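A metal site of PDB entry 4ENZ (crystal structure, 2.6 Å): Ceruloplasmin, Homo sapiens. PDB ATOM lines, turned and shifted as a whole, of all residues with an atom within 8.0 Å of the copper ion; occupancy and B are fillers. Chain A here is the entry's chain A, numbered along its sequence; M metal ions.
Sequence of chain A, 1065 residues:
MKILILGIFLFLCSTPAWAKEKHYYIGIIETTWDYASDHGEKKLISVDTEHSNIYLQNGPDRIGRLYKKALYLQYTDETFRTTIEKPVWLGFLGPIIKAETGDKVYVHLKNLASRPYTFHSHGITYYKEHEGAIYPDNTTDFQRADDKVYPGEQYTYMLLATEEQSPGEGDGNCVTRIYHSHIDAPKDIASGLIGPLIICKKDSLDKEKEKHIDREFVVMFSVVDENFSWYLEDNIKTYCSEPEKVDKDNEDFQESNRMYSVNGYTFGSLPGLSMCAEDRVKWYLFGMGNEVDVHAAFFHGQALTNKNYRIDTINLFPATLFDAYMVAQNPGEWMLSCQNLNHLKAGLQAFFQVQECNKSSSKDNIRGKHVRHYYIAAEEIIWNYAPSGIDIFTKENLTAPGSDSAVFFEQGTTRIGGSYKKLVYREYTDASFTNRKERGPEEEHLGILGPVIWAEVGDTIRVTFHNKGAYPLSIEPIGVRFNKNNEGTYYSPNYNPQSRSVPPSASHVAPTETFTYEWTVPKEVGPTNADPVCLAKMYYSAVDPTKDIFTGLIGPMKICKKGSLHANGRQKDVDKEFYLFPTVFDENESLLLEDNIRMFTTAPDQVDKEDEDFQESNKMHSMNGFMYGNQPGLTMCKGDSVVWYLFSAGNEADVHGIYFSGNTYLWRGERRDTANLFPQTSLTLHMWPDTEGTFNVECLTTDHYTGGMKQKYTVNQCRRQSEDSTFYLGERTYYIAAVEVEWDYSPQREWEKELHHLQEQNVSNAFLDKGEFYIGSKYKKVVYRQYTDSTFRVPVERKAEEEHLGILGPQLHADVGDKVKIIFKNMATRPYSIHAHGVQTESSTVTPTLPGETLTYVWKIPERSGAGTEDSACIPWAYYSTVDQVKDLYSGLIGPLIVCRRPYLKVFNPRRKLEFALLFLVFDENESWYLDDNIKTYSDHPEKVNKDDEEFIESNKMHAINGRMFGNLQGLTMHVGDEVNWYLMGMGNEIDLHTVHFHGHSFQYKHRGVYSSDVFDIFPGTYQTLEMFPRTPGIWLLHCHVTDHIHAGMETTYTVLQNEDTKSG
Leu 993 touches the copper ion.
CG1 of Val 1042 touches the copper ion (3.7 Å).
Met 1050 touches the copper ion (SD to CU, 3.3 Å).
Within 4 Å of the copper ion: Leu 993, His 994, Cys 1040, Val 1042, His 1045 and Met 1050.
The nearest printed residue that does not touch the copper ion is Thr 995 (4.6 Å).
The backbone carbonyl oxygen (O) of Leu 993 lies close to a ring nitrogen (ND1) of His 1045 (3.3 Å).
OD1 of Asp 992 sits at hydrogen-bond distance from NE2 of His 994, 2.6 Å away.
The backbone NH (N) of Thr 995 lies close to the side-chain sulfur (SG) of Cys 1040, 3.3 Å away.
A ring nitrogen (NE2) of His 1045 lies close to the backbone carbonyl oxygen of Ile 991, at 3.5 Å.
The side-chain sulfur (SG) of Cys 1040 lies close to the backbone NH (N) of Val 1042.
N of Cys 1040 is in hydrogen-bond range of O of Met 1050, at 3.4 Å.
The backbone NH of Ile 1018 lies within hydrogen-bond range of the backbone carbonyl oxygen of His 994 (2.7 Å).
The side-chain carboxylate of Glu 291 lies within hydrogen-bond range of a ring nitrogen (NE2) of His 1045 (3.0 Å).
The copper ion is bound by ND1 of His 1045, ND1 of His 994 and SG of Cys 1040.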
ATOM      1  N   GLU A 291     -33.431   1.474 -10.496  1.00  0.00           N
ATOM      2  CA  GLU A 291     -32.742   1.783  -9.219  1.00  0.00           C
ATOM      3  C   GLU A 291     -33.574   1.529  -7.948  1.00  0.00           C
ATOM      4  O   GLU A 291     -33.021   1.290  -6.870  1.00  0.00           O
ATOM      5  CB  GLU A 291     -32.284   3.258  -9.215  1.00  0.00           C
ATOM      6  CG  GLU A 291     -31.100   3.591 -10.162  1.00  0.00           C
ATOM      7  CD  GLU A 291     -30.885   5.097 -10.392  1.00  0.00           C
ATOM      8  OE1 GLU A 291     -29.808   5.478 -10.919  1.00  0.00           O
ATOM      9  OE2 GLU A 291     -31.780   5.913 -10.061  1.00  0.00           O
ATOM     10  N   PHE A 920     -17.728  -0.011 -13.049  1.00  0.00           N
ATOM     11  CA  PHE A 920     -19.061   0.477 -13.255  1.00  0.00           C
ATOM     12  C   PHE A 920     -19.282   1.583 -12.241  1.00  0.00           C
ATOM     13  O   PHE A 920     -19.340   1.333 -11.041  1.00  0.00           O
ATOM     14  CB  PHE A 920     -20.047  -0.683 -13.112  1.00  0.00           C
ATOM     15  CG  PHE A 920     -20.098  -1.529 -14.330  1.00  0.00           C
ATOM     16  CD1 PHE A 920     -19.029  -2.359 -14.649  1.00  0.00           C
ATOM     17  CD2 PHE A 920     -21.139  -1.433 -15.214  1.00  0.00           C
ATOM     18  CE1 PHE A 920     -19.034  -3.116 -15.827  1.00  0.00           C
ATOM     19  CE2 PHE A 920     -21.144  -2.178 -16.387  1.00  0.00           C
ATOM     20  CZ  PHE A 920     -20.091  -3.020 -16.693  1.00  0.00           C
ATOM     21  N   LEU A 921     -19.343   2.824 -12.699  1.00  0.00           N
ATOM     22  CA  LEU A 921     -19.485   3.958 -11.789  1.00  0.00           C
ATOM     23  C   LEU A 921     -20.250   5.049 -12.497  1.00  0.00           C
ATOM     24  O   LEU A 921     -19.996   5.305 -13.677  1.00  0.00           O
ATOM     25  CB  LEU A 921     -18.122   4.514 -11.406  1.00  0.00           C
ATOM     26  CG  LEU A 921     -17.895   5.243 -10.066  1.00  0.00           C
ATOM     27  CD1 LEU A 921     -16.829   6.297 -10.257  1.00  0.00           C
ATOM     28  CD2 LEU A 921     -19.145   5.831  -9.398  1.00  0.00           C
ATOM     29  N   VAL A 922     -21.188   5.656 -11.800  1.00  0.00           N
ATOM     30  CA  VAL A 922     -21.798   6.887 -12.267  1.00  0.00           C
ATOM     31  C   VAL A 922     -20.888   8.039 -11.814  1.00  0.00           C
ATOM     32  O   VAL A 922     -20.828   8.380 -10.648  1.00  0.00           O
ATOM     33  CB  VAL A 922     -23.231   7.063 -11.699  1.00  0.00           C
ATOM     34  CG1 VAL A 922     -23.825   8.349 -12.152  1.00  0.00           C
ATOM     35  CG2 VAL A 922     -24.126   5.874 -12.121  1.00  0.00           C
ATOM     36  N   HIS A 959     -23.125   8.268 -16.458  1.00  0.00           N
ATOM     37  CA  HIS A 959     -23.268   6.836 -16.177  1.00  0.00           C
ATOM     38  C   HIS A 959     -22.360   6.063 -17.088  1.00  0.00           C
ATOM     39  O   HIS A 959     -22.786   5.673 -18.161  1.00  0.00           O
ATOM     40  CB  HIS A 959     -24.702   6.373 -16.449  1.00  0.00           C
ATOM     41  CG  HIS A 959     -25.727   6.971 -15.535  1.00  0.00           C
ATOM     42  ND1 HIS A 959     -25.964   8.337 -15.475  1.00  0.00           N
ATOM     43  CD2 HIS A 959     -26.616   6.394 -14.695  1.00  0.00           C
ATOM     44  CE1 HIS A 959     -26.962   8.562 -14.632  1.00  0.00           C
ATOM     45  NE2 HIS A 959     -27.374   7.404 -14.138  1.00  0.00           N
ATOM     46  N   ALA A 960     -21.138   5.769 -16.644  1.00  0.00           N
ATOM     47  CA  ALA A 960     -20.079   5.268 -17.503  1.00  0.00           C
ATOM     48  C   ALA A 960     -19.539   3.878 -17.107  1.00  0.00           C
ATOM     49  O   ALA A 960     -19.831   3.366 -16.027  1.00  0.00           O
ATOM     50  CB  ALA A 960     -18.964   6.266 -17.471  1.00  0.00           C
ATOM     51  N   ILE A 991     -27.379   4.798  -5.533  1.00  0.00           N
ATOM     52  CA  ILE A 991     -27.683   4.638  -6.942  1.00  0.00           C
ATOM     53  C   ILE A 991     -26.810   3.647  -7.691  1.00  0.00           C
ATOM     54  O   ILE A 991     -27.206   3.076  -8.692  1.00  0.00           O
ATOM     55  CB  ILE A 991     -27.541   6.125  -7.534  1.00  0.00           C
ATOM     56  CG1 ILE A 991     -28.884   6.833  -7.436  1.00  0.00           C
ATOM     57  CG2 ILE A 991     -26.865   6.210  -8.880  1.00  0.00           C
ATOM     58  CD1 ILE A 991     -30.050   5.904  -6.976  1.00  0.00           C
ATOM     59  N   ASP A 992     -25.607   3.428  -7.206  1.00  0.00           N
ATOM     60  CA  ASP A 992     -24.654   2.631  -7.931  1.00  0.00           C
ATOM     61  C   ASP A 992     -24.833   1.130  -7.750  1.00  0.00           C
ATOM     62  O   ASP A 992     -23.907   0.406  -7.426  1.00  0.00           O
ATOM     63  CB  ASP A 992     -23.242   3.094  -7.586  1.00  0.00           C
ATOM     64  CG  ASP A 992     -22.806   4.244  -8.481  1.00  0.00           C
ATOM     65  OD1 ASP A 992     -22.527   3.958  -9.649  1.00  0.00           O
ATOM     66  OD2 ASP A 992     -22.763   5.418  -8.022  1.00  0.00           O
ATOM     67  N   LEU A 993     -26.046   0.662  -7.982  1.00  0.00           N
ATOM     68  CA  LEU A 993     -26.202  -0.762  -8.216  1.00  0.00           C
ATOM     69  C   LEU A 993     -26.116  -1.048  -9.694  1.00  0.00           C
ATOM     70  O   LEU A 993     -26.720  -0.376 -10.522  1.00  0.00           O
ATOM     71  CB  LEU A 993     -27.455  -1.366  -7.591  1.00  0.00           C
ATOM     72  CG  LEU A 993     -28.890  -0.829  -7.464  1.00  0.00           C
ATOM     73  CD1 LEU A 993     -29.002   0.611  -6.998  1.00  0.00           C
ATOM     74  CD2 LEU A 993     -29.629  -1.084  -8.720  1.00  0.00           C
ATOM     75  N   HIS A 994     -25.322  -2.051 -10.014  1.00  0.00           N
ATOM     76  CA  HIS A 994     -25.027  -2.318 -11.364  1.00  0.00           C
ATOM     77  C   HIS A 994     -25.092  -3.824 -11.599  1.00  0.00           C
ATOM     78  O   HIS A 994     -24.359  -4.583 -10.971  1.00  0.00           O
ATOM     79  CB  HIS A 994     -23.609  -1.782 -11.702  1.00  0.00           C
ATOM     80  CG  HIS A 994     -23.453  -0.316 -11.474  1.00  0.00           C
ATOM     81  ND1 HIS A 994     -24.226   0.643 -12.128  1.00  0.00           N
ATOM     82  CD2 HIS A 994     -22.619   0.368 -10.665  1.00  0.00           C
ATOM     83  CE1 HIS A 994     -23.883   1.839 -11.701  1.00  0.00           C
ATOM     84  NE2 HIS A 994     -22.914   1.711 -10.809  1.00  0.00           N
ATOM     85  N   THR A 995     -25.943  -4.243 -12.511  1.00  0.00           N
ATOM     86  CA  THR A 995     -26.059  -5.616 -12.847  1.00  0.00           C
ATOM     87  C   THR A 995     -25.426  -5.866 -14.184  1.00  0.00           C
ATOM     88  O   THR A 995     -26.004  -5.599 -15.201  1.00  0.00           O
ATOM     89  CB  THR A 995     -27.503  -5.964 -12.804  1.00  0.00           C
ATOM     90  OG1 THR A 995     -28.253  -4.978 -13.487  1.00  0.00           O
ATOM     91  CG2 THR A 995     -27.928  -5.940 -11.348  1.00  0.00           C
ATOM     92  N   VAL A 996     -24.201  -6.351 -14.180  1.00  0.00           N
ATOM     93  CA  VAL A 996     -23.385  -6.391 -15.364  1.00  0.00           C
ATOM     94  C   VAL A 996     -23.704  -7.620 -16.172  1.00  0.00           C
ATOM     95  O   VAL A 996     -23.683  -8.765 -15.664  1.00  0.00           O
ATOM     96  CB  VAL A 996     -21.878  -6.368 -15.002  1.00  0.00           C
ATOM     97  CG1 VAL A 996     -21.000  -6.418 -16.256  1.00  0.00           C
ATOM     98  CG2 VAL A 996     -21.581  -5.121 -14.251  1.00  0.00           C
ATOM     99  N   ILE A1018     -22.949  -5.867  -9.073  1.00  0.00           N
ATOM    100  CA  ILE A1018     -21.834  -5.012  -8.671  1.00  0.00           C
ATOM    101  C   ILE A1018     -22.302  -3.801  -7.900  1.00  0.00           C
ATOM    102  O   ILE A1018     -23.185  -3.125  -8.328  1.00  0.00           O
ATOM    103  CB  ILE A1018     -21.031  -4.546  -9.893  1.00  0.00           C
ATOM    104  CG1 ILE A1018     -20.272  -5.734 -10.453  1.00  0.00           C
ATOM    105  CG2 ILE A1018     -20.006  -3.518  -9.541  1.00  0.00           C
ATOM    106  CD1 ILE A1018     -19.362  -6.407  -9.411  1.00  0.00           C
ATOM    107  N   HIS A1039     -23.491  -4.462 -20.951  1.00  0.00           N
ATOM    108  CA  HIS A1039     -24.197  -3.407 -20.257  1.00  0.00           C
ATOM    109  C   HIS A1039     -24.683  -3.789 -18.877  1.00  0.00           C
ATOM    110  O   HIS A1039     -24.783  -4.976 -18.523  1.00  0.00           O
ATOM    111  CB  HIS A1039     -25.381  -2.913 -21.097  1.00  0.00           C
ATOM    112  CG  HIS A1039     -26.512  -3.903 -21.246  1.00  0.00           C
ATOM    113  ND1 HIS A1039     -27.556  -3.993 -20.336  1.00  0.00           N
ATOM    114  CD2 HIS A1039     -26.813  -4.779 -22.253  1.00  0.00           C
ATOM    115  CE1 HIS A1039     -28.420  -4.908 -20.766  1.00  0.00           C
ATOM    116  NE2 HIS A1039     -27.990  -5.400 -21.925  1.00  0.00           N
ATOM    117  N   CYS A1040     -25.008  -2.742 -18.116  1.00  0.00           N
ATOM    118  CA  CYS A1040     -25.755  -2.839 -16.859  1.00  0.00           C
ATOM    119  C   CYS A1040     -27.232  -2.989 -17.184  1.00  0.00           C
ATOM    120  O   CYS A1040     -27.718  -2.338 -18.098  1.00  0.00           O
ATOM    121  CB  CYS A1040     -25.569  -1.557 -16.071  1.00  0.00           C
ATOM    122  SG  CYS A1040     -26.351  -1.634 -14.508  1.00  0.00           S
ATOM    123  N   HIS A1041     -27.956  -3.829 -16.451  1.00  0.00           N
ATOM    124  CA  HIS A1041     -29.315  -4.148 -16.845  1.00  0.00           C
ATOM    125  C   HIS A1041     -30.281  -3.261 -16.061  1.00  0.00           C
ATOM    126  O   HIS A1041     -31.474  -3.457 -16.159  1.00  0.00           O
ATOM    127  CB  HIS A1041     -29.601  -5.646 -16.590  1.00  0.00           C
ATOM    128  CG  HIS A1041     -30.508  -6.330 -17.581  1.00  0.00           C
ATOM    129  ND1 HIS A1041     -31.870  -6.139 -17.625  1.00  0.00           N
ATOM    130  CD2 HIS A1041     -30.240  -7.330 -18.474  1.00  0.00           C
ATOM    131  CE1 HIS A1041     -32.386  -6.944 -18.544  1.00  0.00           C
ATOM    132  NE2 HIS A1041     -31.419  -7.684 -19.068  1.00  0.00           N
ATOM    133  N   VAL A1042     -29.800  -2.311 -15.255  1.00  0.00           N
ATOM    134  CA  VAL A1042     -30.757  -1.377 -14.612  1.00  0.00           C
ATOM    135  C   VAL A1042     -31.240  -0.287 -15.621  1.00  0.00           C
ATOM    136  O   VAL A1042     -30.456   0.448 -16.197  1.00  0.00           O
ATOM    137  CB  VAL A1042     -30.282  -0.805 -13.172  1.00  0.00           C
ATOM    138  CG1 VAL A1042     -28.998  -1.442 -12.715  1.00  0.00           C
ATOM    139  CG2 VAL A1042     -30.231   0.716 -13.090  1.00  0.00           C
ATOM    140  N   THR A1043     -32.559  -0.242 -15.793  1.00  0.00           N
ATOM    141  CA  THR A1043     -33.218   0.680 -16.706  1.00  0.00           C
ATOM    142  C   THR A1043     -32.485   2.011 -16.823  1.00  0.00           C
ATOM    143  O   THR A1043     -31.826   2.277 -17.828  1.00  0.00           O
ATOM    144  CB  THR A1043     -34.675   0.941 -16.290  1.00  0.00           C
ATOM    145  OG1 THR A1043     -35.449  -0.256 -16.449  1.00  0.00           O
ATOM    146  CG2 THR A1043     -35.276   2.056 -17.138  1.00  0.00           C
ATOM    147  N   ASP A1044     -32.606   2.856 -15.809  1.00  0.00           N
ATOM    148  CA  ASP A1044     -32.025   4.206 -15.902  1.00  0.00           C
ATOM    149  C   ASP A1044     -30.592   4.171 -16.385  1.00  0.00           C
ATOM    150  O   ASP A1044     -30.212   4.983 -17.227  1.00  0.00           O
ATOM    151  CB  ASP A1044     -32.105   5.002 -14.593  1.00  0.00           C
ATOM    152  CG  ASP A1044     -33.431   5.741 -14.427  1.00  0.00           C
ATOM    153  OD1 ASP A1044     -33.411   6.764 -13.667  1.00  0.00           O
ATOM    154  OD2 ASP A1044     -34.463   5.350 -15.037  1.00  0.00           O
ATOM    155  N   HIS A1045     -29.809   3.200 -15.911  1.00  0.00           N
ATOM    156  CA  HIS A1045     -28.419   3.086 -16.370  1.00  0.00           C
ATOM    157  C   HIS A1045     -28.260   2.735 -17.882  1.00  0.00           C
ATOM    158  O   HIS A1045     -27.462   3.401 -18.547  1.00  0.00           O
ATOM    159  CB  HIS A1045     -27.580   2.156 -15.458  1.00  0.00           C
ATOM    160  CG  HIS A1045     -27.605   2.542 -14.019  1.00  0.00           C
ATOM    161  ND1 HIS A1045     -27.013   1.776 -13.033  1.00  0.00           N
ATOM    162  CD2 HIS A1045     -28.195   3.593 -13.398  1.00  0.00           C
ATOM    163  CE1 HIS A1045     -27.205   2.368 -11.862  1.00  0.00           C
ATOM    164  NE2 HIS A1045     -27.924   3.465 -12.053  1.00  0.00           N
ATOM    165  N   ILE A1046     -28.973   1.744 -18.435  1.00  0.00           N
ATOM    166  CA  ILE A1046     -28.844   1.457 -19.880  1.00  0.00           C
ATOM    167  C   ILE A1046     -29.120   2.722 -20.662  1.00  0.00           C
ATOM    168  O   ILE A1046     -28.329   3.135 -21.455  1.00  0.00           O
ATOM    169  CB  ILE A1046     -29.857   0.412 -20.456  1.00  0.00           C
ATOM    170  CG1 ILE A1046     -29.940  -0.845 -19.603  1.00  0.00           C
ATOM    171  CG2 ILE A1046     -29.430   0.005 -21.906  1.00  0.00           C
ATOM    172  CD1 ILE A1046     -30.855  -1.969 -20.200  1.00  0.00           C
ATOM    173  N   MET A1050     -24.743   3.366 -20.025  1.00  0.00           N
ATOM    174  CA  MET A1050     -23.784   2.528 -19.313  1.00  0.00           C
ATOM    175  C   MET A1050     -23.693   1.201 -20.064  1.00  0.00           C
ATOM    176  O   MET A1050     -24.279   0.200 -19.675  1.00  0.00           O
ATOM    177  CB  MET A1050     -24.226   2.336 -17.858  1.00  0.00           C
ATOM    178  CG  MET A1050     -23.188   1.716 -16.965  1.00  0.00           C
ATOM    179  SD  MET A1050     -23.561   1.875 -15.210  1.00  0.00           S
ATOM    180  CE  MET A1050     -22.971   3.501 -14.919  1.00  0.00           C
HETATM  181 CU    CU M   1     -25.831   0.258 -13.403  1.00  0.00          CU
